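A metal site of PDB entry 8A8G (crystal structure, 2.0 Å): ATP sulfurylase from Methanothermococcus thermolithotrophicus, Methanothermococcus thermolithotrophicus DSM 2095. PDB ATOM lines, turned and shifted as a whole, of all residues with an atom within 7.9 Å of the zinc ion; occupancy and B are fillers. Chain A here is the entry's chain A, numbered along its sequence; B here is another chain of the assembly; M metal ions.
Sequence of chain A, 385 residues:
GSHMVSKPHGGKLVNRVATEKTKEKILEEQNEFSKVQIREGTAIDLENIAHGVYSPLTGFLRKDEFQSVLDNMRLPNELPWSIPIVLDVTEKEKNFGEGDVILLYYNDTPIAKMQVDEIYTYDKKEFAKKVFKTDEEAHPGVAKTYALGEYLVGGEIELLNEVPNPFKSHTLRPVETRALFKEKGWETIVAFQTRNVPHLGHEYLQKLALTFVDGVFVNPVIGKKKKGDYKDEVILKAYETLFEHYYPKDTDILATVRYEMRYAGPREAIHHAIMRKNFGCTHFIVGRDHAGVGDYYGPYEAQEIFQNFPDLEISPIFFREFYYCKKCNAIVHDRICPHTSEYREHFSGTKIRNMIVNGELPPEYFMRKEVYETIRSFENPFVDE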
ATOM      1  N   TYR A 323     -29.211  12.207  16.894  1.00  0.00           N
ATOM      2  CA  TYR A 323     -30.129  12.993  17.757  1.00  0.00           C
ATOM      3  C   TYR A 323     -29.310  14.020  18.531  1.00  0.00           C
ATOM      4  O   TYR A 323     -28.112  13.806  18.703  1.00  0.00           O
ATOM      5  CB  TYR A 323     -30.853  12.059  18.734  1.00  0.00           C
ATOM      6  CG  TYR A 323     -29.920  11.210  19.564  1.00  0.00           C
ATOM      7  CD1 TYR A 323     -29.363  11.709  20.729  1.00  0.00           C
ATOM      8  CD2 TYR A 323     -29.611   9.917  19.190  1.00  0.00           C
ATOM      9  CE1 TYR A 323     -28.504  10.934  21.499  1.00  0.00           C
ATOM     10  CE2 TYR A 323     -28.758   9.133  19.952  1.00  0.00           C
ATOM     11  CZ  TYR A 323     -28.206   9.644  21.118  1.00  0.00           C
ATOM     12  OH  TYR A 323     -27.372   8.881  21.865  1.00  0.00           O
ATOM     13  N   TYR A 324     -29.943  15.126  18.916  1.00  0.00           N
ATOM     14  CA  TYR A 324     -29.216  16.103  19.747  1.00  0.00           C
ATOM     15  C   TYR A 324     -29.172  15.562  21.171  1.00  0.00           C
ATOM     16  O   TYR A 324     -30.191  15.039  21.648  1.00  0.00           O
ATOM     17  CB  TYR A 324     -29.867  17.484  19.719  1.00  0.00           C
ATOM     18  CG  TYR A 324     -29.080  18.504  20.512  1.00  0.00           C
ATOM     19  CD1 TYR A 324     -28.008  19.166  19.949  1.00  0.00           C
ATOM     20  CD2 TYR A 324     -29.367  18.751  21.838  1.00  0.00           C
ATOM     21  CE1 TYR A 324     -27.266  20.079  20.673  1.00  0.00           C
ATOM     22  CE2 TYR A 324     -28.638  19.666  22.583  1.00  0.00           C
ATOM     23  CZ  TYR A 324     -27.579  20.338  21.991  1.00  0.00           C
ATOM     24  OH  TYR A 324     -26.852  21.236  22.707  1.00  0.00           O
ATOM     25  N   CYS A 325     -28.019  15.659  21.828  1.00  0.00           N
ATOM     26  CA  CYS A 325     -27.915  15.183  23.222  1.00  0.00           C
ATOM     27  C   CYS A 325     -27.695  16.388  24.131  1.00  0.00           C
ATOM     28  O   CYS A 325     -26.742  17.139  23.888  1.00  0.00           O
ATOM     29  CB  CYS A 325     -26.782  14.194  23.403  1.00  0.00           C
ATOM     30  SG  CYS A 325     -26.594  13.722  25.135  1.00  0.00           S
ATOM     31  N   LYS A 326     -28.518  16.528  25.165  1.00  0.00           N
ATOM     32  CA  LYS A 326     -28.437  17.685  26.037  1.00  0.00           C
ATOM     33  C   LYS A 326     -27.407  17.544  27.149  1.00  0.00           C
ATOM     34  O   LYS A 326     -27.291  18.460  27.968  1.00  0.00           O
ATOM     35  CB  LYS A 326     -29.801  17.963  26.670  1.00  0.00           C
ATOM     36  CG  LYS A 326     -30.828  18.355  25.620  1.00  0.00           C
ATOM     37  CD  LYS A 326     -32.175  18.671  26.241  1.00  0.00           C
ATOM     38  CE  LYS A 326     -32.973  17.408  26.505  1.00  0.00           C
ATOM     39  NZ  LYS A 326     -34.410  17.775  26.839  1.00  0.00           N
ATOM     40  N   LYS A 327     -26.692  16.425  27.215  1.00  0.00           N
ATOM     41  CA  LYS A 327     -25.492  16.366  28.050  1.00  0.00           C
ATOM     42  C   LYS A 327     -24.210  16.391  27.232  1.00  0.00           C
ATOM     43  O   LYS A 327     -23.263  17.107  27.591  1.00  0.00           O
ATOM     44  CB  LYS A 327     -25.537  15.119  28.922  1.00  0.00           C
ATOM     45  CG  LYS A 327     -24.282  14.921  29.722  1.00  0.00           C
ATOM     46  CD  LYS A 327     -24.533  14.003  30.900  1.00  0.00           C
ATOM     47  CE  LYS A 327     -23.296  13.883  31.763  1.00  0.00           C
ATOM     48  NZ  LYS A 327     -23.646  13.255  33.089  1.00  0.00           N
ATOM     49  N   CYS A 328     -24.154  15.676  26.116  1.00  0.00           N
ATOM     50  CA  CYS A 328     -23.044  15.854  25.192  1.00  0.00           C
ATOM     51  C   CYS A 328     -23.064  17.270  24.609  1.00  0.00           C
ATOM     52  O   CYS A 328     -22.018  17.790  24.233  1.00  0.00           O
ATOM     53  CB  CYS A 328     -23.078  14.802  24.092  1.00  0.00           C
ATOM     54  SG  CYS A 328     -22.770  13.075  24.652  1.00  0.00           S
ATOM     55  N   ASN A 329     -24.239  17.899  24.546  1.00  0.00           N
ATOM     56  CA  ASN A 329     -24.398  19.235  23.952  1.00  0.00           C
ATOM     57  C   ASN A 329     -24.028  19.241  22.466  1.00  0.00           C
ATOM     58  O   ASN A 329     -23.323  20.118  21.962  1.00  0.00           O
ATOM     59  CB  ASN A 329     -23.575  20.278  24.713  1.00  0.00           C
ATOM     60  CG  ASN A 329     -24.035  20.425  26.160  1.00  0.00           C
ATOM     61  OD1 ASN A 329     -25.203  20.206  26.478  1.00  0.00           O
ATOM     62  ND2 ASN A 329     -23.098  20.790  27.042  1.00  0.00           N
ATOM     63  N   ALA A 330     -24.527  18.253  21.742  1.00  0.00           N
ATOM     64  CA  ALA A 330     -24.073  18.058  20.378  1.00  0.00           C
ATOM     65  C   ALA A 330     -25.003  17.068  19.690  1.00  0.00           C
ATOM     66  O   ALA A 330     -25.710  16.293  20.331  1.00  0.00           O
ATOM     67  CB  ALA A 330     -22.628  17.575  20.355  1.00  0.00           C
ATOM     68  N   VAL A 332     -25.308  13.773  18.075  1.00  0.00           N
ATOM     69  CA  VAL A 332     -24.498  12.590  18.302  1.00  0.00           C
ATOM     70  C   VAL A 332     -25.238  11.377  17.777  1.00  0.00           C
ATOM     71  O   VAL A 332     -26.301  11.508  17.173  1.00  0.00           O
ATOM     72  CB  VAL A 332     -24.164  12.439  19.802  1.00  0.00           C
ATOM     73  CG1 VAL A 332     -23.330  13.578  20.267  1.00  0.00           C
ATOM     74  CG2 VAL A 332     -25.435  12.372  20.576  1.00  0.00           C
ATOM     75  N   HIS A 333     -24.682  10.188  18.045  1.00  0.00           N
ATOM     76  CA  HIS A 333     -25.338   8.906  17.694  1.00  0.00           C
ATOM     77  C   HIS A 333     -25.162   7.925  18.863  1.00  0.00           C
ATOM     78  O   HIS A 333     -24.326   8.198  19.737  1.00  0.00           O
ATOM     79  CB  HIS A 333     -24.941   8.382  16.299  1.00  0.00           C
ATOM     80  CG  HIS A 333     -23.480   8.439  15.997  1.00  0.00           C
ATOM     81  ND1 HIS A 333     -22.689   7.315  15.976  1.00  0.00           N
ATOM     82  CD2 HIS A 333     -22.687   9.481  15.671  1.00  0.00           C
ATOM     83  CE1 HIS A 333     -21.456   7.657  15.665  1.00  0.00           C
ATOM     84  NE2 HIS A 333     -21.427   8.974  15.480  1.00  0.00           N
ATOM     85  N   ILE A 336     -21.587   6.669  20.152  1.00  0.00           N
ATOM     86  CA  ILE A 336     -20.650   7.539  20.895  1.00  0.00           C
ATOM     87  C   ILE A 336     -21.293   8.252  22.073  1.00  0.00           C
ATOM     88  O   ILE A 336     -20.610   9.036  22.741  1.00  0.00           O
ATOM     89  CB  ILE A 336     -19.988   8.578  19.966  1.00  0.00           C
ATOM     90  CG1 ILE A 336     -21.056   9.452  19.319  1.00  0.00           C
ATOM     91  CG2 ILE A 336     -19.073   7.921  18.942  1.00  0.00           C
ATOM     92  CD1 ILE A 336     -20.456  10.660  18.637  1.00  0.00           C
ATOM     93  N   CYS A 337     -22.578   8.057  22.327  1.00  0.00           N
ATOM     94  CA  CYS A 337     -23.271   8.700  23.414  1.00  0.00           C
ATOM     95  C   CYS A 337     -23.923   7.649  24.287  1.00  0.00           C
ATOM     96  O   CYS A 337     -24.622   6.774  23.793  1.00  0.00           O
ATOM     97  CB  CYS A 337     -24.360   9.651  22.874  1.00  0.00           C
ATOM     98  SG  CYS A 337     -25.498  10.232  24.102  1.00  0.00           S
ATOM     99  N   PRO A 338     -23.626   7.657  25.596  1.00  0.00           N
ATOM    100  CA  PRO A 338     -24.208   6.639  26.503  1.00  0.00           C
ATOM    101  C   PRO A 338     -25.396   7.108  27.308  1.00  0.00           C
ATOM    102  O   PRO A 338     -25.819   6.372  28.209  1.00  0.00           O
ATOM    103  CB  PRO A 338     -23.020   6.397  27.439  1.00  0.00           C
ATOM    104  CG  PRO A 338     -22.497   7.780  27.620  1.00  0.00           C
ATOM    105  CD  PRO A 338     -22.630   8.476  26.300  1.00  0.00           C
ATOM    106  N   HIS A 339     -25.954   8.280  27.011  1.00  0.00           N
ATOM    107  CA  HIS A 339     -26.917   8.922  27.883  1.00  0.00           C
ATOM    108  C   HIS A 339     -28.338   8.458  27.627  1.00  0.00           C
ATOM    109  O   HIS A 339     -28.709   8.045  26.532  1.00  0.00           O
ATOM    110  CB  HIS A 339     -26.835  10.435  27.720  1.00  0.00           C
ATOM    111  CG  HIS A 339     -25.482  10.969  28.023  1.00  0.00           C
ATOM    112  ND1 HIS A 339     -24.793  11.772  27.147  1.00  0.00           N
ATOM    113  CD2 HIS A 339     -24.698  10.816  29.112  1.00  0.00           C
ATOM    114  CE1 HIS A 339     -23.621  12.087  27.689  1.00  0.00           C
ATOM    115  NE2 HIS A 339     -23.551  11.524  28.887  1.00  0.00           N
ATOM    116  N   THR A 340     -29.127   8.544  28.684  1.00  0.00           N
ATOM    117  CA  THR A 340     -30.455   7.977  28.694  1.00  0.00           C
ATOM    118  C   THR A 340     -31.444   8.902  27.996  1.00  0.00           C
ATOM    119  O   THR A 340     -31.110  10.022  27.579  1.00  0.00           O
ATOM    120  CB  THR A 340     -30.829   7.673  30.131  1.00  0.00           C
ATOM    121  OG1 THR A 340     -30.721   8.849  30.940  1.00  0.00           O
ATOM    122  CG2 THR A 340     -29.882   6.665  30.710  1.00  0.00           C
ATOM    123  N   TYR A 343     -32.125  12.936  27.925  1.00  0.00           N
ATOM    124  CA  TYR A 343     -31.142  13.822  27.332  1.00  0.00           C
ATOM    125  C   TYR A 343     -31.222  13.879  25.812  1.00  0.00           C
ATOM    126  O   TYR A 343     -30.602  14.762  25.231  1.00  0.00           O
ATOM    127  CB  TYR A 343     -29.733  13.396  27.755  1.00  0.00           C
ATOM    128  CG  TYR A 343     -29.485  13.531  29.240  1.00  0.00           C
ATOM    129  CD1 TYR A 343     -29.196  14.764  29.800  1.00  0.00           C
ATOM    130  CD2 TYR A 343     -29.543  12.440  30.066  1.00  0.00           C
ATOM    131  CE1 TYR A 343     -28.976  14.885  31.156  1.00  0.00           C
ATOM    132  CE2 TYR A 343     -29.305  12.546  31.429  1.00  0.00           C
ATOM    133  CZ  TYR A 343     -29.045  13.773  31.966  1.00  0.00           C
ATOM    134  OH  TYR A 343     -28.821  13.889  33.301  1.00  0.00           O
ATOM    135  N   ARG A 344     -31.958  12.962  25.180  1.00  0.00           N
ATOM    136  CA  ARG A 344     -31.979  12.806  23.737  1.00  0.00           C
ATOM    137  C   ARG A 344     -33.158  13.553  23.137  1.00  0.00           C
ATOM    138  O   ARG A 344     -34.293  13.428  23.614  1.00  0.00           O
ATOM    139  CB  ARG A 344     -32.060  11.335  23.334  1.00  0.00           C
ATOM    140  CG  ARG A 344     -30.978  10.506  23.961  1.00  0.00           C
ATOM    141  CD  ARG A 344     -30.822   9.133  23.314  1.00  0.00           C
ATOM    142  NE  ARG A 344     -29.692   8.442  23.940  1.00  0.00           N
ATOM    143  CZ  ARG A 344     -29.135   7.316  23.507  1.00  0.00           C
ATOM    144  NH1 ARG A 344     -29.608   6.663  22.450  1.00  0.00           N
ATOM    145  NH2 ARG A 344     -28.073   6.820  24.139  1.00  0.00           N
ATOM    146  N   GLU B 203     -11.788  14.655  22.957  1.00  0.00           N
ATOM    147  CA  GLU B 203     -12.973  13.811  22.886  1.00  0.00           C
ATOM    148  C   GLU B 203     -13.505  13.733  21.454  1.00  0.00           C
ATOM    149  O   GLU B 203     -13.888  12.668  20.997  1.00  0.00           O
ATOM    150  CB  GLU B 203     -14.018  14.354  23.835  1.00  0.00           C
ATOM    151  CG  GLU B 203     -15.296  13.562  23.958  1.00  0.00           C
ATOM    152  CD  GLU B 203     -16.240  14.214  24.959  1.00  0.00           C
ATOM    153  OE1 GLU B 203     -15.769  15.112  25.722  1.00  0.00           O
ATOM    154  OE2 GLU B 203     -17.439  13.846  24.981  1.00  0.00           O
ATOM    155  N   LYS B 207     -13.922  10.090  19.627  1.00  0.00           N
ATOM    156  CA  LYS B 207     -15.231   9.598  19.207  1.00  0.00           C
ATOM    157  C   LYS B 207     -15.397   9.624  17.701  1.00  0.00           C
ATOM    158  O   LYS B 207     -16.208   8.883  17.146  1.00  0.00           O
ATOM    159  CB  LYS B 207     -16.332  10.431  19.868  1.00  0.00           C
ATOM    160  CG  LYS B 207     -16.378  10.262  21.400  1.00  0.00           C
ATOM    161  CD  LYS B 207     -17.506  11.036  22.044  1.00  0.00           C
ATOM    162  CE  LYS B 207     -17.709  10.623  23.490  1.00  0.00           C
ATOM    163  NZ  LYS B 207     -18.788  11.442  24.089  1.00  0.00           N
ATOM    164  N   HIS B 245     -18.754   9.681  32.355  1.00  0.00           N
ATOM    165  CA  HIS B 245     -19.866  10.586  32.118  1.00  0.00           C
ATOM    166  C   HIS B 245     -20.199  10.777  30.654  1.00  0.00           C
ATOM    167  O   HIS B 245     -21.316  11.198  30.350  1.00  0.00           O
ATOM    168  CB  HIS B 245     -19.588  11.954  32.736  1.00  0.00           C
ATOM    169  CG  HIS B 245     -19.830  12.006  34.203  1.00  0.00           C
ATOM    170  ND1 HIS B 245     -21.050  12.349  34.734  1.00  0.00           N
ATOM    171  CD2 HIS B 245     -19.027  11.745  35.256  1.00  0.00           C
ATOM    172  CE1 HIS B 245     -20.990  12.296  36.055  1.00  0.00           C
ATOM    173  NE2 HIS B 245     -19.777  11.927  36.387  1.00  0.00           N
ATOM    174  N   TYR B 246     -19.277  10.474  29.744  1.00  0.00           N
ATOM    175  CA  TYR B 246     -19.505  10.784  28.353  1.00  0.00           C
ATOM    176  C   TYR B 246     -19.202   9.677  27.366  1.00  0.00           C
ATOM    177  O   TYR B 246     -19.426   9.851  26.171  1.00  0.00           O
ATOM    178  CB  TYR B 246     -18.680  12.027  27.991  1.00  0.00           C
ATOM    179  CG  TYR B 246     -19.187  13.241  28.698  1.00  0.00           C
ATOM    180  CD1 TYR B 246     -18.731  13.585  29.953  1.00  0.00           C
ATOM    181  CD2 TYR B 246     -20.144  14.057  28.100  1.00  0.00           C
ATOM    182  CE1 TYR B 246     -19.230  14.716  30.623  1.00  0.00           C
ATOM    183  CE2 TYR B 246     -20.634  15.193  28.757  1.00  0.00           C
ATOM    184  CZ  TYR B 246     -20.191  15.493  30.017  1.00  0.00           C
ATOM    185  OH  TYR B 246     -20.644  16.621  30.669  1.00  0.00           O
ATOM    186  N   TYR B 247     -18.719   8.525  27.806  1.00  0.00           N
ATOM    187  CA  TYR B 247     -18.381   7.474  26.886  1.00  0.00           C
ATOM    188  C   TYR B 247     -19.162   6.195  27.173  1.00  0.00           C
ATOM    189  O   TYR B 247     -19.329   5.820  28.331  1.00  0.00           O
ATOM    190  CB  TYR B 247     -16.902   7.139  26.989  1.00  0.00           C
ATOM    191  CG  TYR B 247     -15.972   8.124  26.338  1.00  0.00           C
ATOM    192  CD1 TYR B 247     -15.900   9.444  26.758  1.00  0.00           C
ATOM    193  CD2 TYR B 247     -15.117   7.719  25.315  1.00  0.00           C
ATOM    194  CE1 TYR B 247     -15.026  10.326  26.172  1.00  0.00           C
ATOM    195  CE2 TYR B 247     -14.226   8.587  24.737  1.00  0.00           C
ATOM    196  CZ  TYR B 247     -14.188   9.883  25.162  1.00  0.00           C
ATOM    197  OH  TYR B 247     -13.305  10.746  24.569  1.00  0.00           O
ATOM    198  N   ARG B 368     -15.519  19.650  29.810  1.00  0.00           N
ATOM    199  CA  ARG B 368     -16.749  19.063  30.414  1.00  0.00           C
ATOM    200  C   ARG B 368     -16.828  19.508  31.878  1.00  0.00           C
ATOM    201  O   ARG B 368     -15.792  19.397  32.566  1.00  0.00           O
ATOM    202  CB  ARG B 368     -16.737  17.537  30.293  1.00  0.00           C
ATOM    203  CG  ARG B 368     -16.706  17.024  28.853  1.00  0.00           C
ATOM    204  CD  ARG B 368     -17.942  17.416  28.087  1.00  0.00           C
ATOM    205  NE  ARG B 368     -18.139  16.592  26.889  1.00  0.00           N
ATOM    206  CZ  ARG B 368     -19.082  16.798  25.989  1.00  0.00           C
ATOM    207  NH1 ARG B 368     -19.933  17.795  26.124  1.00  0.00           N
ATOM    208  NH2 ARG B 368     -19.177  15.991  24.940  1.00  0.00           N
HETATM  209 ZN    ZN M   1     -24.853  12.207  25.097  1.00  0.00          ZN
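Within 4 Å of the zinc ion: Cys 325, Cys 328, Cys 337 and His 339.
The backbone carbonyl oxygen (O) of Ala 330 is in hydrogen-bond range of the backbone NH (N) of Cys 325. NE2 of His 339 is in hydrogen-bond range of O of His 245 of chain B, 2.7 Å away. N of Lys 327 sits close to SG of Cys 325, 3.4 Å away. The side-chain sulfur (SG) of Cys 337 lies close to the side-chain hydroxyl (OH) of Tyr 323, 3.2 Å away. The backbone carbonyl oxygen (O) of Cys 337 is in hydrogen-bond range of the guanidinium group (NH2) of Arg 344. NH1 of Arg 368 of chain B sits at hydrogen-bond distance from O of Cys 328, at 2.8 Å. The guanidinium group (NH2) of Arg 344 lies within hydrogen-bond range of the backbone carbonyl oxygen (O) of His 339 (2.8 Å).
The zinc ion is bound by ND1 of His 339 (2.1 Å), SG of Cys 328 (2.3 Å), SG of Cys 337 (2.3 Å) and SG of Cys 325 (2.3 Å). The zinc ion has four donor atoms within binding distance.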
